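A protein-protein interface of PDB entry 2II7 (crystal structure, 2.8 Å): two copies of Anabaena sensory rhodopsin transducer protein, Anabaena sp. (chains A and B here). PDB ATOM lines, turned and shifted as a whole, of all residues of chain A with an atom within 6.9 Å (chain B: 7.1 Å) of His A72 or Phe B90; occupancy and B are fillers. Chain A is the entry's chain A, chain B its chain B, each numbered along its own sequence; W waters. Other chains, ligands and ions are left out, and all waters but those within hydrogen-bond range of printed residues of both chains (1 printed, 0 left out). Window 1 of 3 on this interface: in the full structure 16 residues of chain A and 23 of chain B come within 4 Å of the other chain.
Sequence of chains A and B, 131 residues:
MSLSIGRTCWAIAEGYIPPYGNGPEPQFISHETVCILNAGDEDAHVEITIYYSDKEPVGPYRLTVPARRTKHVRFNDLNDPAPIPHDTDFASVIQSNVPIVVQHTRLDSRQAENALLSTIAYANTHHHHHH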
ATOM      1  N   THR A  33     -24.357 -38.472  -3.629  1.00  0.00           N
ATOM      2  CA  THR A  33     -24.161 -37.989  -2.272  1.00  0.00           C
ATOM      3  C   THR A  33     -25.113 -36.870  -1.879  1.00  0.00           C
ATOM      4  O   THR A  33     -25.533 -36.055  -2.704  1.00  0.00           O
ATOM      5  CB  THR A  33     -22.727 -37.484  -2.050  1.00  0.00           C
ATOM      6  OG1 THR A  33     -21.797 -38.466  -2.521  1.00  0.00           O
ATOM      7  CG2 THR A  33     -22.482 -37.234  -0.564  1.00  0.00           C
ATOM      8  N   VAL A  34     -25.450 -36.856  -0.597  1.00  0.00           N
ATOM      9  CA  VAL A  34     -26.322 -35.850  -0.028  1.00  0.00           C
ATOM     10  C   VAL A  34     -25.462 -35.089   0.952  1.00  0.00           C
ATOM     11  O   VAL A  34     -25.101 -35.616   1.996  1.00  0.00           O
ATOM     12  CB  VAL A  34     -27.475 -36.485   0.742  1.00  0.00           C
ATOM     13  CG1 VAL A  34     -28.250 -35.425   1.495  1.00  0.00           C
ATOM     14  CG2 VAL A  34     -28.374 -37.195  -0.211  1.00  0.00           C
ATOM     15  N   CYS A  35     -25.115 -33.859   0.615  1.00  0.00           N
ATOM     16  CA  CYS A  35     -24.293 -33.081   1.513  1.00  0.00           C
ATOM     17  C   CYS A  35     -25.202 -32.285   2.422  1.00  0.00           C
ATOM     18  O   CYS A  35     -26.117 -31.609   1.966  1.00  0.00           O
ATOM     19  CB  CYS A  35     -23.376 -32.179   0.706  1.00  0.00           C
ATOM     20  SG  CYS A  35     -22.347 -33.149  -0.409  1.00  0.00           S
ATOM     21  N   ILE A  36     -24.964 -32.389   3.720  1.00  0.00           N
ATOM     22  CA  ILE A  36     -25.782 -31.675   4.682  1.00  0.00           C
ATOM     23  C   ILE A  36     -24.944 -30.758   5.545  1.00  0.00           C
ATOM     24  O   ILE A  36     -23.797 -31.064   5.872  1.00  0.00           O
ATOM     25  CB  ILE A  36     -26.514 -32.638   5.616  1.00  0.00           C
ATOM     26  CG1 ILE A  36     -27.295 -33.668   4.801  1.00  0.00           C
ATOM     27  CG2 ILE A  36     -27.424 -31.860   6.542  1.00  0.00           C
ATOM     28  CD1 ILE A  36     -28.020 -34.688   5.653  1.00  0.00           C
ATOM     29  N   LEU A  63     -29.853 -40.905  11.199  1.00  0.00           N
ATOM     30  CA  LEU A  63     -28.485 -40.423  11.054  1.00  0.00           C
ATOM     31  C   LEU A  63     -28.391 -39.088  11.800  1.00  0.00           C
ATOM     32  O   LEU A  63     -29.394 -38.400  11.962  1.00  0.00           O
ATOM     33  CB  LEU A  63     -28.217 -40.263   9.550  1.00  0.00           C
ATOM     34  CG  LEU A  63     -27.215 -39.343   8.862  1.00  0.00           C
ATOM     35  CD1 LEU A  63     -27.406 -39.516   7.348  1.00  0.00           C
ATOM     36  CD2 LEU A  63     -27.435 -37.890   9.257  1.00  0.00           C
ATOM     37  N   THR A  70     -20.775 -30.311   9.142  1.00  0.00           N
ATOM     38  CA  THR A  70     -21.305 -30.693   7.840  1.00  0.00           C
ATOM     39  C   THR A  70     -21.189 -32.203   7.776  1.00  0.00           C
ATOM     40  O   THR A  70     -20.599 -32.819   8.664  1.00  0.00           O
ATOM     41  CB  THR A  70     -20.484 -30.106   6.685  1.00  0.00           C
ATOM     42  OG1 THR A  70     -21.015 -30.568   5.440  1.00  0.00           O
ATOM     43  CG2 THR A  70     -19.058 -30.549   6.774  1.00  0.00           C
ATOM     44  N   LYS A  71     -21.746 -32.808   6.737  1.00  0.00           N
ATOM     45  CA  LYS A  71     -21.673 -34.255   6.609  1.00  0.00           C
ATOM     46  C   LYS A  71     -22.190 -34.745   5.277  1.00  0.00           C
ATOM     47  O   LYS A  71     -23.360 -34.572   4.942  1.00  0.00           O
ATOM     48  CB  LYS A  71     -22.458 -34.936   7.729  1.00  0.00           C
ATOM     49  CG  LYS A  71     -22.380 -36.462   7.706  1.00  0.00           C
ATOM     50  CD  LYS A  71     -22.946 -37.053   8.998  1.00  0.00           C
ATOM     51  CE  LYS A  71     -22.685 -38.551   9.110  1.00  0.00           C
ATOM     52  NZ  LYS A  71     -23.157 -39.088  10.423  1.00  0.00           N
ATOM     53  N   HIS A  72     -21.301 -35.356   4.512  1.00  0.00           N
ATOM     54  CA  HIS A  72     -21.665 -35.894   3.219  1.00  0.00           C
ATOM     55  C   HIS A  72     -22.135 -37.317   3.427  1.00  0.00           C
ATOM     56  O   HIS A  72     -21.506 -38.094   4.144  1.00  0.00           O
ATOM     57  CB  HIS A  72     -20.462 -35.849   2.290  1.00  0.00           C
ATOM     58  CG  HIS A  72     -19.993 -34.458   2.007  1.00  0.00           C
ATOM     59  ND1 HIS A  72     -20.161 -33.421   2.903  1.00  0.00           N
ATOM     60  CD2 HIS A  72     -19.342 -33.933   0.941  1.00  0.00           C
ATOM     61  CE1 HIS A  72     -19.632 -32.317   2.403  1.00  0.00           C
ATOM     62  NE2 HIS A  72     -19.129 -32.602   1.214  1.00  0.00           N
ATOM     63  N   VAL A  73     -23.255 -37.650   2.809  1.00  0.00           N
ATOM     64  CA  VAL A  73     -23.809 -38.975   2.953  1.00  0.00           C
ATOM     65  C   VAL A  73     -23.976 -39.626   1.597  1.00  0.00           C
ATOM     66  O   VAL A  73     -24.719 -39.131   0.756  1.00  0.00           O
ATOM     67  CB  VAL A  73     -25.169 -38.908   3.660  1.00  0.00           C
ATOM     68  CG1 VAL A  73     -25.766 -40.303   3.791  1.00  0.00           C
ATOM     69  CG2 VAL A  73     -25.002 -38.253   5.020  1.00  0.00           C
ATOM     70  N   ARG A  74     -23.258 -40.724   1.383  1.00  0.00           N
ATOM     71  CA  ARG A  74     -23.351 -41.472   0.135  1.00  0.00           C
ATOM     72  C   ARG A  74     -24.604 -42.315   0.250  1.00  0.00           C
ATOM     73  O   ARG A  74     -24.807 -42.998   1.253  1.00  0.00           O
ATOM     74  CB  ARG A  74     -22.145 -42.392  -0.041  1.00  0.00           C
ATOM     75  CG  ARG A  74     -20.863 -41.680  -0.393  1.00  0.00           C
ATOM     76  CD  ARG A  74     -19.666 -42.504   0.032  1.00  0.00           C
ATOM     77  NE  ARG A  74     -18.434 -42.004  -0.562  1.00  0.00           N
ATOM     78  CZ  ARG A  74     -18.106 -42.197  -1.832  1.00  0.00           C
ATOM     79  NH1 ARG A  74     -18.926 -42.883  -2.614  1.00  0.00           N
ATOM     80  NH2 ARG A  74     -16.972 -41.706  -2.318  1.00  0.00           N
ATOM     81  N   ILE B  12     -23.603 -23.485   1.192  1.00  0.00           N
ATOM     82  CA  ILE B  12     -23.241 -24.525   0.231  1.00  0.00           C
ATOM     83  C   ILE B  12     -22.874 -25.764   1.045  1.00  0.00           C
ATOM     84  O   ILE B  12     -21.864 -25.788   1.732  1.00  0.00           O
ATOM     85  CB  ILE B  12     -22.063 -24.077  -0.653  1.00  0.00           C
ATOM     86  CG1 ILE B  12     -22.423 -22.765  -1.338  1.00  0.00           C
ATOM     87  CG2 ILE B  12     -21.783 -25.099  -1.721  1.00  0.00           C
ATOM     88  CD1 ILE B  12     -21.360 -22.229  -2.237  1.00  0.00           C
ATOM     89  N   ALA B  13     -23.717 -26.786   0.975  1.00  0.00           N
ATOM     90  CA  ALA B  13     -23.512 -28.018   1.728  1.00  0.00           C
ATOM     91  C   ALA B  13     -22.381 -28.891   1.185  1.00  0.00           C
ATOM     92  O   ALA B  13     -21.820 -29.710   1.910  1.00  0.00           O
ATOM     93  CB  ALA B  13     -24.817 -28.818   1.773  1.00  0.00           C
ATOM     94  N   GLU B  14     -22.052 -28.728  -0.088  1.00  0.00           N
ATOM     95  CA  GLU B  14     -20.981 -29.509  -0.682  1.00  0.00           C
ATOM     96  C   GLU B  14     -19.690 -28.700  -0.698  1.00  0.00           C
ATOM     97  O   GLU B  14     -19.709 -27.472  -0.702  1.00  0.00           O
ATOM     98  CB  GLU B  14     -21.361 -29.944  -2.108  1.00  0.00           C
ATOM     99  CG  GLU B  14     -20.239 -30.658  -2.892  1.00  0.00           C
ATOM    100  CD  GLU B  14     -19.696 -31.912  -2.200  1.00  0.00           C
ATOM    101  OE1 GLU B  14     -19.176 -31.793  -1.070  1.00  0.00           O
ATOM    102  OE2 GLU B  14     -19.782 -33.012  -2.794  1.00  0.00           O
ATOM    103  N   GLY B  15     -18.569 -29.404  -0.695  1.00  0.00           N
ATOM    104  CA  GLY B  15     -17.274 -28.756  -0.715  1.00  0.00           C
ATOM    105  C   GLY B  15     -16.178 -29.806  -0.741  1.00  0.00           C
ATOM    106  O   GLY B  15     -16.087 -30.638   0.171  1.00  0.00           O
ATOM    107  N   TYR B  16     -15.338 -29.771  -1.776  1.00  0.00           N
ATOM    108  CA  TYR B  16     -14.265 -30.752  -1.894  1.00  0.00           C
ATOM    109  C   TYR B  16     -13.182 -30.400  -2.902  1.00  0.00           C
ATOM    110  O   TYR B  16     -13.464 -30.147  -4.073  1.00  0.00           O
ATOM    111  CB  TYR B  16     -14.854 -32.100  -2.282  1.00  0.00           C
ATOM    112  CG  TYR B  16     -13.846 -33.212  -2.330  1.00  0.00           C
ATOM    113  CD1 TYR B  16     -13.421 -33.839  -1.163  1.00  0.00           C
ATOM    114  CD2 TYR B  16     -13.325 -33.656  -3.547  1.00  0.00           C
ATOM    115  CE1 TYR B  16     -12.507 -34.885  -1.207  1.00  0.00           C
ATOM    116  CE2 TYR B  16     -12.403 -34.705  -3.603  1.00  0.00           C
ATOM    117  CZ  TYR B  16     -12.004 -35.313  -2.428  1.00  0.00           C
ATOM    118  OH  TYR B  16     -11.103 -36.348  -2.471  1.00  0.00           O
ATOM    119  N   ILE B  17     -11.938 -30.388  -2.437  1.00  0.00           N
ATOM    120  CA  ILE B  17     -10.793 -30.120  -3.305  1.00  0.00           C
ATOM    121  C   ILE B  17     -10.026 -31.453  -3.372  1.00  0.00           C
ATOM    122  O   ILE B  17      -9.389 -31.861  -2.401  1.00  0.00           O
ATOM    123  CB  ILE B  17      -9.884 -29.033  -2.714  1.00  0.00           C
ATOM    124  CG1 ILE B  17     -10.716 -27.817  -2.312  1.00  0.00           C
ATOM    125  CG2 ILE B  17      -8.862 -28.619  -3.746  1.00  0.00           C
ATOM    126  CD1 ILE B  17      -9.910 -26.692  -1.679  1.00  0.00           C
ATOM    127  N   GLU B  32     -13.637 -26.313  -7.860  1.00  0.00           N
ATOM    128  CA  GLU B  32     -14.807 -25.857  -7.113  1.00  0.00           C
ATOM    129  C   GLU B  32     -14.732 -24.382  -6.802  1.00  0.00           C
ATOM    130  O   GLU B  32     -13.961 -23.934  -5.959  1.00  0.00           O
ATOM    131  CB  GLU B  32     -14.959 -26.655  -5.827  1.00  0.00           C
ATOM    132  CG  GLU B  32     -16.304 -26.496  -5.196  1.00  0.00           C
ATOM    133  CD  GLU B  32     -16.571 -27.566  -4.169  1.00  0.00           C
ATOM    134  OE1 GLU B  32     -16.512 -28.762  -4.531  1.00  0.00           O
ATOM    135  OE2 GLU B  32     -16.841 -27.211  -3.003  1.00  0.00           O
ATOM    136  N   THR B  49     -17.383 -18.744   5.750  1.00  0.00           N
ATOM    137  CA  THR B  49     -17.097 -19.621   6.861  1.00  0.00           C
ATOM    138  C   THR B  49     -17.101 -21.053   6.335  1.00  0.00           C
ATOM    139  O   THR B  49     -18.043 -21.470   5.661  1.00  0.00           O
ATOM    140  CB  THR B  49     -18.171 -19.494   7.934  1.00  0.00           C
ATOM    141  OG1 THR B  49     -18.204 -18.142   8.405  1.00  0.00           O
ATOM    142  CG2 THR B  49     -17.889 -20.439   9.081  1.00  0.00           C
ATOM    143  N   ILE B  50     -16.046 -21.803   6.633  1.00  0.00           N
ATOM    144  CA  ILE B  50     -15.961 -23.179   6.179  1.00  0.00           C
ATOM    145  C   ILE B  50     -16.284 -24.107   7.334  1.00  0.00           C
ATOM    146  O   ILE B  50     -15.789 -23.933   8.443  1.00  0.00           O
ATOM    147  CB  ILE B  50     -14.559 -23.512   5.638  1.00  0.00           C
ATOM    148  CG1 ILE B  50     -14.149 -22.498   4.564  1.00  0.00           C
ATOM    149  CG2 ILE B  50     -14.556 -24.912   5.024  1.00  0.00           C
ATOM    150  CD1 ILE B  50     -14.966 -22.584   3.289  1.00  0.00           C
ATOM    151  N   TYR B  51     -17.141 -25.085   7.069  1.00  0.00           N
ATOM    152  CA  TYR B  51     -17.540 -26.052   8.077  1.00  0.00           C
ATOM    153  C   TYR B  51     -16.985 -27.423   7.710  1.00  0.00           C
ATOM    154  O   TYR B  51     -16.828 -27.750   6.534  1.00  0.00           O
ATOM    155  CB  TYR B  51     -19.070 -26.125   8.177  1.00  0.00           C
ATOM    156  CG  TYR B  51     -19.738 -24.896   8.775  1.00  0.00           C
ATOM    157  CD1 TYR B  51     -19.846 -23.704   8.050  1.00  0.00           C
ATOM    158  CD2 TYR B  51     -20.254 -24.925  10.070  1.00  0.00           C
ATOM    159  CE1 TYR B  51     -20.452 -22.575   8.601  1.00  0.00           C
ATOM    160  CE2 TYR B  51     -20.860 -23.797  10.632  1.00  0.00           C
ATOM    161  CZ  TYR B  51     -20.952 -22.626   9.891  1.00  0.00           C
ATOM    162  OH  TYR B  51     -21.518 -21.505  10.458  1.00  0.00           O
ATOM    163  N   TYR B  52     -16.684 -28.226   8.723  1.00  0.00           N
ATOM    164  CA  TYR B  52     -16.139 -29.562   8.492  1.00  0.00           C
ATOM    165  C   TYR B  52     -17.004 -30.596   9.182  1.00  0.00           C
ATOM    166  O   TYR B  52     -17.921 -30.254   9.939  1.00  0.00           O
ATOM    167  CB  TYR B  52     -14.694 -29.647   9.008  1.00  0.00           C
ATOM    168  CG  TYR B  52     -13.732 -28.741   8.259  1.00  0.00           C
ATOM    169  CD1 TYR B  52     -13.218 -29.115   7.014  1.00  0.00           C
ATOM    170  CD2 TYR B  52     -13.388 -27.481   8.758  1.00  0.00           C
ATOM    171  CE1 TYR B  52     -12.396 -28.259   6.284  1.00  0.00           C
ATOM    172  CE2 TYR B  52     -12.569 -26.620   8.036  1.00  0.00           C
ATOM    173  CZ  TYR B  52     -12.078 -27.008   6.797  1.00  0.00           C
ATOM    174  OH  TYR B  52     -11.318 -26.124   6.044  1.00  0.00           O
ATOM    175  N   SER B  53     -16.707 -31.862   8.922  1.00  0.00           N
ATOM    176  CA  SER B  53     -17.469 -32.957   9.509  1.00  0.00           C
ATOM    177  C   SER B  53     -16.973 -33.434  10.875  1.00  0.00           C
ATOM    178  O   SER B  53     -17.686 -34.157  11.572  1.00  0.00           O
ATOM    179  CB  SER B  53     -17.486 -34.138   8.542  1.00  0.00           C
ATOM    180  OG  SER B  53     -16.169 -34.465   8.139  1.00  0.00           O
ATOM    181  N   PHE B  75     -12.191 -21.989  -4.011  1.00  0.00           N
ATOM    182  CA  PHE B  75     -12.022 -22.337  -2.612  1.00  0.00           C
ATOM    183  C   PHE B  75     -10.554 -22.626  -2.316  1.00  0.00           C
ATOM    184  O   PHE B  75     -10.047 -22.300  -1.242  1.00  0.00           O
ATOM    185  CB  PHE B  75     -12.856 -23.573  -2.273  1.00  0.00           C
ATOM    186  CG  PHE B  75     -14.287 -23.270  -1.928  1.00  0.00           C
ATOM    187  CD1 PHE B  75     -14.596 -22.553  -0.780  1.00  0.00           C
ATOM    188  CD2 PHE B  75     -15.331 -23.718  -2.738  1.00  0.00           C
ATOM    189  CE1 PHE B  75     -15.923 -22.286  -0.439  1.00  0.00           C
ATOM    190  CE2 PHE B  75     -16.660 -23.456  -2.405  1.00  0.00           C
ATOM    191  CZ  PHE B  75     -16.958 -22.738  -1.252  1.00  0.00           C
ATOM    192  N   ASN B  76      -9.876 -23.246  -3.274  1.00  0.00           N
ATOM    193  CA  ASN B  76      -8.467 -23.586  -3.117  1.00  0.00           C
ATOM    194  C   ASN B  76      -7.614 -22.345  -2.857  1.00  0.00           C
ATOM    195  O   ASN B  76      -6.645 -22.397  -2.099  1.00  0.00           O
ATOM    196  CB  ASN B  76      -7.964 -24.303  -4.370  1.00  0.00           C
ATOM    197  CG  ASN B  76      -6.574 -24.857  -4.197  1.00  0.00           C
ATOM    198  OD1 ASN B  76      -5.640 -24.132  -3.853  1.00  0.00           O
ATOM    199  ND2 ASN B  76      -6.425 -26.150  -4.434  1.00  0.00           N
ATOM    200  N   LEU B  78      -8.362 -19.888  -1.179  1.00  0.00           N
ATOM    201  CA  LEU B  78      -8.586 -19.353   0.161  1.00  0.00           C
ATOM    202  C   LEU B  78      -7.398 -19.759   1.023  1.00  0.00           C
ATOM    203  O   LEU B  78      -6.931 -20.890   0.929  1.00  0.00           O
ATOM    204  CB  LEU B  78      -9.899 -19.908   0.736  1.00  0.00           C
ATOM    205  CG  LEU B  78     -11.173 -19.040   0.670  1.00  0.00           C
ATOM    206  CD1 LEU B  78     -11.284 -18.261  -0.638  1.00  0.00           C
ATOM    207  CD2 LEU B  78     -12.374 -19.952   0.856  1.00  0.00           C
ATOM    208  N   ILE B  84      -7.730 -24.442   2.963  1.00  0.00           N
ATOM    209  CA  ILE B  84      -8.665 -25.542   3.146  1.00  0.00           C
ATOM    210  C   ILE B  84      -7.967 -26.870   2.862  1.00  0.00           C
ATOM    211  O   ILE B  84      -7.412 -27.078   1.779  1.00  0.00           O
ATOM    212  CB  ILE B  84      -9.930 -25.393   2.219  1.00  0.00           C
ATOM    213  CG1 ILE B  84     -10.856 -24.286   2.739  1.00  0.00           C
ATOM    214  CG2 ILE B  84     -10.725 -26.698   2.181  1.00  0.00           C
ATOM    215  CD1 ILE B  84     -10.308 -22.893   2.584  1.00  0.00           C
ATOM    216  N   PRO B  85      -7.979 -27.782   3.845  1.00  0.00           N
ATOM    217  CA  PRO B  85      -7.362 -29.109   3.744  1.00  0.00           C
ATOM    218  C   PRO B  85      -7.867 -29.824   2.507  1.00  0.00           C
ATOM    219  O   PRO B  85      -9.079 -29.994   2.358  1.00  0.00           O
ATOM    220  CB  PRO B  85      -7.845 -29.814   5.008  1.00  0.00           C
ATOM    221  CG  PRO B  85      -8.014 -28.696   5.992  1.00  0.00           C
ATOM    222  CD  PRO B  85      -8.626 -27.593   5.159  1.00  0.00           C
ATOM    223  N   THR B  88     -10.815 -33.281   1.590  1.00  0.00           N
ATOM    224  CA  THR B  88     -11.619 -33.188   2.800  1.00  0.00           C
ATOM    225  C   THR B  88     -12.990 -32.634   2.441  1.00  0.00           C
ATOM    226  O   THR B  88     -13.091 -31.613   1.754  1.00  0.00           O
ATOM    227  CB  THR B  88     -10.988 -32.236   3.838  1.00  0.00           C
ATOM    228  OG1 THR B  88      -9.628 -32.610   4.079  1.00  0.00           O
ATOM    229  CG2 THR B  88     -11.760 -32.297   5.148  1.00  0.00           C
ATOM    230  N   ASP B  89     -14.042 -33.310   2.892  1.00  0.00           N
ATOM    231  CA  ASP B  89     -15.392 -32.847   2.616  1.00  0.00           C
ATOM    232  C   ASP B  89     -15.703 -31.671   3.531  1.00  0.00           C
ATOM    233  O   ASP B  89     -15.585 -31.781   4.756  1.00  0.00           O
ATOM    234  CB  ASP B  89     -16.421 -33.958   2.856  1.00  0.00           C
ATOM    235  CG  ASP B  89     -16.387 -35.041   1.787  1.00  0.00           C
ATOM    236  OD1 ASP B  89     -16.196 -34.731   0.589  1.00  0.00           O
ATOM    237  OD2 ASP B  89     -16.581 -36.212   2.152  1.00  0.00           O
ATOM    238  N   PHE B  90     -16.075 -30.539   2.936  1.00  0.00           N
ATOM    239  CA  PHE B  90     -16.427 -29.359   3.714  1.00  0.00           C
ATOM    240  C   PHE B  90     -17.707 -28.727   3.168  1.00  0.00           C
ATOM    241  O   PHE B  90     -18.265 -29.186   2.166  1.00  0.00           O
ATOM    242  CB  PHE B  90     -15.285 -28.326   3.713  1.00  0.00           C
ATOM    243  CG  PHE B  90     -14.978 -27.738   2.357  1.00  0.00           C
ATOM    244  CD1 PHE B  90     -14.185 -28.422   1.441  1.00  0.00           C
ATOM    245  CD2 PHE B  90     -15.481 -26.490   1.995  1.00  0.00           C
ATOM    246  CE1 PHE B  90     -13.894 -27.866   0.171  1.00  0.00           C
ATOM    247  CE2 PHE B  90     -15.199 -25.927   0.735  1.00  0.00           C
ATOM    248  CZ  PHE B  90     -14.400 -26.623  -0.180  1.00  0.00           C
ATOM    249  N   ALA B  91     -18.166 -27.688   3.855  1.00  0.00           N
ATOM    250  CA  ALA B  91     -19.355 -26.950   3.479  1.00  0.00           C
ATOM    251  C   ALA B  91     -19.044 -25.501   3.810  1.00  0.00           C
ATOM    252  O   ALA B  91     -18.126 -25.236   4.580  1.00  0.00           O
ATOM    253  CB  ALA B  91     -20.546 -27.423   4.279  1.00  0.00           C
ATOM    254  N   SER B  92     -19.805 -24.568   3.241  1.00  0.00           N
ATOM    255  CA  SER B  92     -19.563 -23.162   3.491  1.00  0.00           C
ATOM    256  C   SER B  92     -20.814 -22.309   3.619  1.00  0.00           C
ATOM    257  O   SER B  92     -21.905 -22.701   3.199  1.00  0.00           O
ATOM    258  CB  SER B  92     -18.684 -22.598   2.384  1.00  0.00           C
ATOM    259  OG  SER B  92     -19.224 -22.877   1.101  1.00  0.00           O
HETATM  260  O   HOH W   1     -18.176 -35.944   5.164  1.00  0.00           O
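OE2 of Glu B14 sits close to SG of Cys A35, 3.5 Å away.
The backbone NH of Thr A70 is in hydrogen-bond range of the backbone carbonyl oxygen of Tyr B52.
A ring nitrogen (NE2) of His A72 lies within hydrogen-bond range of the side-chain carboxylate (OE1) of Glu B14, at 2.4 Å.
SG of Cys A35 lies close to NE2 of His A72, 3.6 Å away.
The backbone carbonyl oxygen of Ile A36 sits at hydrogen-bond distance from the side-chain hydroxyl of Thr A70 (2.9 Å).
The backbone carbonyl oxygen (O) of Gly B15 lies within hydrogen-bond range of the backbone NH (N) of Phe B90, at 2.8 Å.
The backbone carbonyl oxygen (O) of Ala B91 sits at hydrogen-bond distance from the backbone NH (N) of Tyr B51 (2.7 Å).
Among the printed residues, pairs that only touch across the chains: Cys A35 with Ala B13, Thr A70 with Ala B13, Thr A70 with Tyr B51, Thr A70 with Ser B53, Thr A70 with Ala B91, His A72 with Ala B13, His A72 with Gly B15, His A72 with Asp B89 and His A72 with Phe B90.
His A72 touches just these residues of chain B: Ala B13, Glu B14, Gly B15, Asp B89 and Phe B90.
Phe B90 touches one residue of chain A.
Printed residues of chain A within 4 Å of Tyr B52: Thr A70 (3.0 Å).
Of the printed residues of chain A, Tyr B51 touches Thr A70.
Printed residues of chain A within 4 Å of Ser B53: Thr A70 (3.2 Å).
Printed residues of chain A within 4 Å of Ala B13: Cys A35, Thr A70 and His A72.
Printed residues of chain B within 4 Å of Cys A35: Ala B13 (3.1 Å) and Glu B14 (3.4 Å).
Arg A74 touches none of the printed residues of chain B.
Ile B50 touches none of the printed residues of chain A.
The nearest residue of chain A that does not touch Phe B90 is Thr A70 (4.2 Å).
Of the 10 printed residues of chain A, 3 touch a printed residue of chain B.
Hydrophobic or aromatic side chains of chain B within 4 Å of the printed part of chain A: Ala B13 and Ala B91.
Along chain B the printed residues that touch a printed residue of chain A span positions 13 to 91.
Among the printed residues, 12 pairs touch across the chains.
No position is printed for both chains.
Water W1 lies within hydrogen-bond range of the backbone NH of His A72 and the side-chain carboxylate of Asp B89.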
